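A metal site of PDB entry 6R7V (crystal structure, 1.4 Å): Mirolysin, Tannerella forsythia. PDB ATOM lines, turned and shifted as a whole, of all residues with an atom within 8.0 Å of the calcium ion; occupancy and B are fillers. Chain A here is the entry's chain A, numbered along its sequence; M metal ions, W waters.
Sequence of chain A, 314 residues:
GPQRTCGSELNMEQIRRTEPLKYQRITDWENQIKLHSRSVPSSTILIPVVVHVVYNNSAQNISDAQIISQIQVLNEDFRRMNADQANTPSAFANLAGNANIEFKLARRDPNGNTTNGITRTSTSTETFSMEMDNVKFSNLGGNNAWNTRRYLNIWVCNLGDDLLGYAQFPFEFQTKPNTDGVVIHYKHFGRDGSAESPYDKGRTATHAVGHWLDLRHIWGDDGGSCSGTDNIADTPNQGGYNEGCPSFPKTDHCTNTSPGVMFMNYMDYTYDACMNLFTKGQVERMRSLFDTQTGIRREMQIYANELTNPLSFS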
ATOM      1  N   HIS A 217       1.555  10.193  -4.683  1.00  0.00           N
ATOM      2  CA  HIS A 217       0.172   9.889  -5.036  1.00  0.00           C
ATOM      3  C   HIS A 217      -0.465  11.065  -5.747  1.00  0.00           C
ATOM      4  O   HIS A 217      -0.315  12.212  -5.308  1.00  0.00           O
ATOM      5  CB  HIS A 217      -0.611   9.550  -3.798  1.00  0.00           C
ATOM      6  CG  HIS A 217      -0.206   8.238  -3.231  1.00  0.00           C
ATOM      7  ND1 HIS A 217      -0.259   8.000  -1.890  1.00  0.00           N
ATOM      8  CD2 HIS A 217       0.281   7.146  -3.857  1.00  0.00           C
ATOM      9  CE1 HIS A 217       0.162   6.757  -1.720  1.00  0.00           C
ATOM     10  NE2 HIS A 217       0.544   6.212  -2.863  1.00  0.00           N
ATOM     11  N   ILE A 218      -1.177  10.768  -6.830  1.00  0.00           N
ATOM     12  CA  ILE A 218      -1.674  11.810  -7.738  1.00  0.00           C
ATOM     13  C   ILE A 218      -2.682  12.759  -7.048  1.00  0.00           C
ATOM     14  O   ILE A 218      -2.783  13.934  -7.412  1.00  0.00           O
ATOM     15  CB  ILE A 218      -2.280  11.142  -8.986  1.00  0.00           C
ATOM     16  CG1 ILE A 218      -2.614  12.177 -10.062  1.00  0.00           C
ATOM     17  CG2 ILE A 218      -3.512  10.264  -8.636  1.00  0.00           C
ATOM     18  CD1 ILE A 218      -2.840  11.545 -11.440  1.00  0.00           C
ATOM     19  N   TRP A 219      -3.407  12.266  -6.042  1.00  0.00           N
ATOM     20  CA  TRP A 219      -4.397  13.102  -5.357  1.00  0.00           C
ATOM     21  C   TRP A 219      -3.805  13.954  -4.217  1.00  0.00           C
ATOM     22  O   TRP A 219      -4.551  14.725  -3.577  1.00  0.00           O
ATOM     23  CB  TRP A 219      -5.571  12.261  -4.841  1.00  0.00           C
ATOM     24  CG  TRP A 219      -5.217  11.390  -3.690  1.00  0.00           C
ATOM     25  CD1 TRP A 219      -5.362  11.672  -2.360  1.00  0.00           C
ATOM     26  CD2 TRP A 219      -4.597  10.098  -3.765  1.00  0.00           C
ATOM     27  NE1 TRP A 219      -4.857  10.632  -1.610  1.00  0.00           N
ATOM     28  CE2 TRP A 219      -4.402   9.651  -2.434  1.00  0.00           C
ATOM     29  CE3 TRP A 219      -4.254   9.241  -4.821  1.00  0.00           C
ATOM     30  CZ2 TRP A 219      -3.829   8.402  -2.147  1.00  0.00           C
ATOM     31  CZ3 TRP A 219      -3.681   8.014  -4.527  1.00  0.00           C
ATOM     32  CH2 TRP A 219      -3.497   7.594  -3.192  1.00  0.00           C
ATOM     33  N   GLY A 220      -2.512  13.835  -3.931  1.00  0.00           N
ATOM     34  CA  GLY A 220      -1.883  14.700  -2.943  1.00  0.00           C
ATOM     35  C   GLY A 220      -1.923  14.300  -1.488  1.00  0.00           C
ATOM     36  O   GLY A 220      -1.512  15.089  -0.639  1.00  0.00           O
ATOM     37  N   ASP A 221      -2.387  13.078  -1.188  1.00  0.00           N
ATOM     38  CA  ASP A 221      -2.414  12.511   0.160  1.00  0.00           C
ATOM     39  C   ASP A 221      -3.012  13.499   1.139  1.00  0.00           C
ATOM     40  O   ASP A 221      -2.431  13.778   2.188  1.00  0.00           O
ATOM     41  CB  ASP A 221      -0.962  12.137   0.576  1.00  0.00           C
ATOM     42  CG  ASP A 221      -0.441  10.932  -0.164  1.00  0.00           C
ATOM     43  OD1 ASP A 221      -1.151   9.923  -0.211  1.00  0.00           O
ATOM     44  OD2 ASP A 221       0.694  11.004  -0.711  1.00  0.00           O
ATOM     45  N   ASP A 222      -4.182  14.071   0.807  1.00  0.00           N
ATOM     46  CA  ASP A 222      -4.742  15.142   1.611  1.00  0.00           C
ATOM     47  C   ASP A 222      -6.138  14.856   2.090  1.00  0.00           C
ATOM     48  O   ASP A 222      -6.882  15.800   2.418  1.00  0.00           O
ATOM     49  CB  ASP A 222      -4.720  16.419   0.773  1.00  0.00           C
ATOM     50  CG  ASP A 222      -5.360  16.278  -0.606  1.00  0.00           C
ATOM     51  OD1 ASP A 222      -6.030  15.257  -0.857  1.00  0.00           O
ATOM     52  OD2 ASP A 222      -5.174  17.175  -1.434  1.00  0.00           O
ATOM     53  N   GLY A 223      -6.526  13.597   2.079  1.00  0.00           N
ATOM     54  CA  GLY A 223      -7.823  13.196   2.601  1.00  0.00           C
ATOM     55  C   GLY A 223      -9.013  13.625   1.773  1.00  0.00           C
ATOM     56  O   GLY A 223     -10.112  13.724   2.301  1.00  0.00           O
ATOM     57  N   GLY A 224      -8.775  13.911   0.502  1.00  0.00           N
ATOM     58  CA  GLY A 224      -9.853  14.298  -0.390  1.00  0.00           C
ATOM     59  C   GLY A 224      -9.960  15.763  -0.731  1.00  0.00           C
ATOM     60  O   GLY A 224     -10.817  16.135  -1.535  1.00  0.00           O
ATOM     61  N   SER A 225      -9.141  16.612  -0.096  1.00  0.00           N
ATOM     62  CA  SER A 225      -9.204  18.025  -0.398  1.00  0.00           C
ATOM     63  C   SER A 225      -8.504  18.341  -1.729  1.00  0.00           C
ATOM     64  O   SER A 225      -8.055  17.427  -2.418  1.00  0.00           O
ATOM     65  CB  SER A 225      -8.616  18.865   0.736  1.00  0.00           C
ATOM     66  OG  SER A 225      -7.197  18.786   0.702  1.00  0.00           O
ATOM     67  N   CYS A 226      -8.431  19.636  -2.110  1.00  0.00           N
ATOM     68  CA  CYS A 226      -7.749  20.083  -3.325  1.00  0.00           C
ATOM     69  C   CYS A 226      -6.492  20.833  -2.942  1.00  0.00           C
ATOM     70  O   CYS A 226      -5.897  21.523  -3.783  1.00  0.00           O
ATOM     71  CB  CYS A 226      -8.662  20.953  -4.187  1.00  0.00           C
ATOM     72  SG  CYS A 226     -10.282  20.224  -4.504  1.00  0.00           S
ATOM     73  N   SER A 227      -6.077  20.731  -1.693  1.00  0.00           N
ATOM     74  CA  SER A 227      -4.962  21.500  -1.163  1.00  0.00           C
ATOM     75  C   SER A 227      -3.628  20.843  -1.325  1.00  0.00           C
ATOM     76  O   SER A 227      -2.626  21.549  -1.448  1.00  0.00           O
ATOM     77  CB  SER A 227      -5.183  21.843   0.301  1.00  0.00           C
ATOM     78  OG  SER A 227      -5.383  20.663   1.075  1.00  0.00           O
ATOM     79  N   GLY A 228      -3.609  19.498  -1.275  1.00  0.00           N
ATOM     80  CA  GLY A 228      -2.400  18.722  -1.443  1.00  0.00           C
ATOM     81  C   GLY A 228      -2.001  18.683  -2.895  1.00  0.00           C
ATOM     82  O   GLY A 228      -2.798  18.993  -3.784  1.00  0.00           O
ATOM     83  N   THR A 229      -0.755  18.328  -3.149  1.00  0.00           N
ATOM     84  CA  THR A 229      -0.270  18.307  -4.532  1.00  0.00           C
ATOM     85  C   THR A 229       0.678  17.171  -4.722  1.00  0.00           C
ATOM     86  O   THR A 229       1.294  16.730  -3.756  1.00  0.00           O
ATOM     87  CB  THR A 229       0.440  19.638  -4.863  1.00  0.00           C
ATOM     88  OG1 THR A 229       0.885  19.630  -6.226  1.00  0.00           O
ATOM     89  CG2 THR A 229       1.625  19.937  -3.925  1.00  0.00           C
ATOM     90  N   ASP A 230       0.800  16.693  -5.978  1.00  0.00           N
ATOM     91  CA  ASP A 230       1.829  15.708  -6.312  1.00  0.00           C
ATOM     92  C   ASP A 230       3.012  16.427  -6.956  1.00  0.00           C
ATOM     93  O   ASP A 230       3.958  15.781  -7.391  1.00  0.00           O
ATOM     94  CB  ASP A 230       1.269  14.574  -7.195  1.00  0.00           C
ATOM     95  CG  ASP A 230       0.847  14.978  -8.590  1.00  0.00           C
ATOM     96  OD1 ASP A 230       0.658  16.198  -8.831  1.00  0.00           O
ATOM     97  OD2 ASP A 230       0.700  14.071  -9.445  1.00  0.00           O
ATOM     98  N   PRO A 236      -3.949  16.350 -13.429  1.00  0.00           N
ATOM     99  CA  PRO A 236      -5.037  17.211 -12.921  1.00  0.00           C
ATOM    100  C   PRO A 236      -5.155  17.164 -11.399  1.00  0.00           C
ATOM    101  O   PRO A 236      -5.019  16.086 -10.824  1.00  0.00           O
ATOM    102  CB  PRO A 236      -6.288  16.615 -13.551  1.00  0.00           C
ATOM    103  CG  PRO A 236      -5.799  15.922 -14.807  1.00  0.00           C
ATOM    104  CD  PRO A 236      -4.441  15.383 -14.444  1.00  0.00           C
ATOM    105  N   ASN A 237      -5.428  18.323 -10.764  1.00  0.00           N
ATOM    106  CA  ASN A 237      -5.671  18.398  -9.330  1.00  0.00           C
ATOM    107  C   ASN A 237      -6.803  17.446  -9.004  1.00  0.00           C
ATOM    108  O   ASN A 237      -7.815  17.399  -9.708  1.00  0.00           O
ATOM    109  CB  ASN A 237      -6.021  19.814  -8.901  1.00  0.00           C
ATOM    110  CG  ASN A 237      -5.999  20.061  -7.423  1.00  0.00           C
ATOM    111  OD1 ASN A 237      -5.818  19.169  -6.603  1.00  0.00           O
ATOM    112  ND2 ASN A 237      -6.182  21.314  -7.038  1.00  0.00           N
ATOM    113  N   GLN A 238      -6.619  16.640  -7.993  1.00  0.00           N
ATOM    114  CA  GLN A 238      -7.558  15.569  -7.718  1.00  0.00           C
ATOM    115  C   GLN A 238      -7.896  15.552  -6.232  1.00  0.00           C
ATOM    116  O   GLN A 238      -7.019  15.801  -5.422  1.00  0.00           O
ATOM    117  CB  GLN A 238      -6.883  14.240  -8.172  1.00  0.00           C
ATOM    118  CG  GLN A 238      -7.688  12.957  -7.938  1.00  0.00           C
ATOM    119  CD  GLN A 238      -7.048  11.745  -8.566  1.00  0.00           C
ATOM    120  OE1 GLN A 238      -6.471  11.779  -9.645  1.00  0.00           O
ATOM    121  NE2 GLN A 238      -7.129  10.628  -7.888  1.00  0.00           N
ATOM    122  N   GLY A 239      -9.154  15.266  -5.885  1.00  0.00           N
ATOM    123  CA  GLY A 239      -9.596  15.226  -4.478  1.00  0.00           C
ATOM    124  C   GLY A 239      -8.950  14.080  -3.718  1.00  0.00           C
ATOM    125  O   GLY A 239      -7.899  14.252  -3.093  1.00  0.00           O
ATOM    126  N   GLY A 240      -9.593  12.925  -3.770  1.00  0.00           N
ATOM    127  CA  GLY A 240      -9.116  11.730  -3.107  1.00  0.00           C
ATOM    128  C   GLY A 240      -8.666  10.679  -4.084  1.00  0.00           C
ATOM    129  O   GLY A 240      -8.629  10.906  -5.309  1.00  0.00           O
ATOM    130  N   TYR A 241      -8.258   9.541  -3.585  1.00  0.00           N
ATOM    131  CA  TYR A 241      -7.833   8.464  -4.444  1.00  0.00           C
ATOM    132  C   TYR A 241      -9.015   7.839  -5.131  1.00  0.00           C
ATOM    133  O   TYR A 241     -10.163   7.949  -4.692  1.00  0.00           O
ATOM    134  CB  TYR A 241      -7.056   7.370  -3.651  1.00  0.00           C
ATOM    135  CG  TYR A 241      -7.840   6.725  -2.515  1.00  0.00           C
ATOM    136  CD1 TYR A 241      -7.588   7.079  -1.180  1.00  0.00           C
ATOM    137  CD2 TYR A 241      -8.811   5.762  -2.763  1.00  0.00           C
ATOM    138  CE1 TYR A 241      -8.318   6.502  -0.135  1.00  0.00           C
ATOM    139  CE2 TYR A 241      -9.546   5.194  -1.716  1.00  0.00           C
ATOM    140  CZ  TYR A 241      -9.313   5.587  -0.413  1.00  0.00           C
ATOM    141  OH  TYR A 241     -10.011   5.013   0.637  1.00  0.00           O
ATOM    142  N   ASP A 252     -14.350  15.525 -10.287  1.00  0.00           N
ATOM    143  CA  ASP A 252     -14.514  15.665  -8.840  1.00  0.00           C
ATOM    144  C   ASP A 252     -14.545  17.158  -8.465  1.00  0.00           C
ATOM    145  O   ASP A 252     -14.577  17.983  -9.375  1.00  0.00           O
ATOM    146  CB  ASP A 252     -13.465  14.861  -8.042  1.00  0.00           C
ATOM    147  CG  ASP A 252     -12.012  15.284  -8.125  1.00  0.00           C
ATOM    148  OD1 ASP A 252     -11.731  16.390  -8.642  1.00  0.00           O
ATOM    149  OD2 ASP A 252     -11.152  14.505  -7.639  1.00  0.00           O
ATOM    150  N   HIS A 253     -14.533  17.513  -7.176  1.00  0.00           N
ATOM    151  CA  HIS A 253     -14.623  18.926  -6.797  1.00  0.00           C
ATOM    152  C   HIS A 253     -13.318  19.719  -7.094  1.00  0.00           C
ATOM    153  O   HIS A 253     -13.384  20.944  -7.137  1.00  0.00           O
ATOM    154  CB  HIS A 253     -15.068  19.108  -5.331  1.00  0.00           C
ATOM    155  CG  HIS A 253     -14.118  18.634  -4.274  1.00  0.00           C
ATOM    156  ND1 HIS A 253     -13.804  19.439  -3.189  1.00  0.00           N
ATOM    157  CD2 HIS A 253     -13.541  17.424  -4.100  1.00  0.00           C
ATOM    158  CE1 HIS A 253     -13.012  18.704  -2.409  1.00  0.00           C
ATOM    159  NE2 HIS A 253     -12.812  17.498  -2.933  1.00  0.00           N
ATOM    160  N   CYS A 254     -12.177  19.036  -7.367  1.00  0.00           N
ATOM    161  CA  CYS A 254     -10.907  19.718  -7.683  1.00  0.00           C
ATOM    162  C   CYS A 254     -10.775  20.028  -9.158  1.00  0.00           C
ATOM    163  O   CYS A 254     -10.278  21.104  -9.491  1.00  0.00           O
ATOM    164  CB  CYS A 254      -9.725  18.912  -7.192  1.00  0.00           C
ATOM    165  SG  CYS A 254      -9.821  18.482  -5.438  1.00  0.00           S
HETATM  166 CA    CA M   1      -6.353  16.067  -3.134  1.00  0.00          CA
HETATM  167  O   HOH W   1      -5.233  17.793  -4.331  1.00  0.00           O
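Five residues have an atom within 4 Å of the calcium ion: Trp 219, Asp 222, Ser 225, Gln 238 and Gly 239. The nearest printed residue that does not touch the calcium ion is Cys 226 (4.3 Å).
The side-chain hydroxyl of Ser 225 sits at hydrogen-bond distance from the side-chain hydroxyl of Ser 227 (2.6 Å). N of Gly 224 sits close to OD1 of Asp 222 (3.3 Å). OD2 of Asp 222 sits close to N of Gly 228, at 2.8 Å. The backbone NH of Gly 239 sits at hydrogen-bond distance from the side-chain sulfur of Cys 254 (3.3 Å). The side-chain carboxylate (OD2) of Asp 252 is in hydrogen-bond range of the backbone NH (N) of Gly 239 (2.8 Å). The side-chain amide nitrogen of Gln 238 sits at hydrogen-bond distance from the backbone carbonyl oxygen of Gly 240, at 3.0 Å. The side-chain sulfur (SG) of Cys 226 forms a disulfide with the side-chain sulfur (SG) of Cys 254, 2.0 Å away.
The calcium ion is bound by the backbone carbonyl oxygen (O) of Trp 219, the backbone carbonyl oxygen (O) of Ser 225, the side-chain carboxylate (OD2) of Asp 222, water W1, the backbone carbonyl oxygen (O) of Gly 239, the backbone carbonyl oxygen (O) of Gln 238 and the side-chain carboxylate (OD1) of Asp 222. The calcium ion has seven donor atoms within binding distance.
Water W1 lies within hydrogen-bond range of OD1 of Asn 237 (2.7 Å) and O of Gly 228 (2.8 Å).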
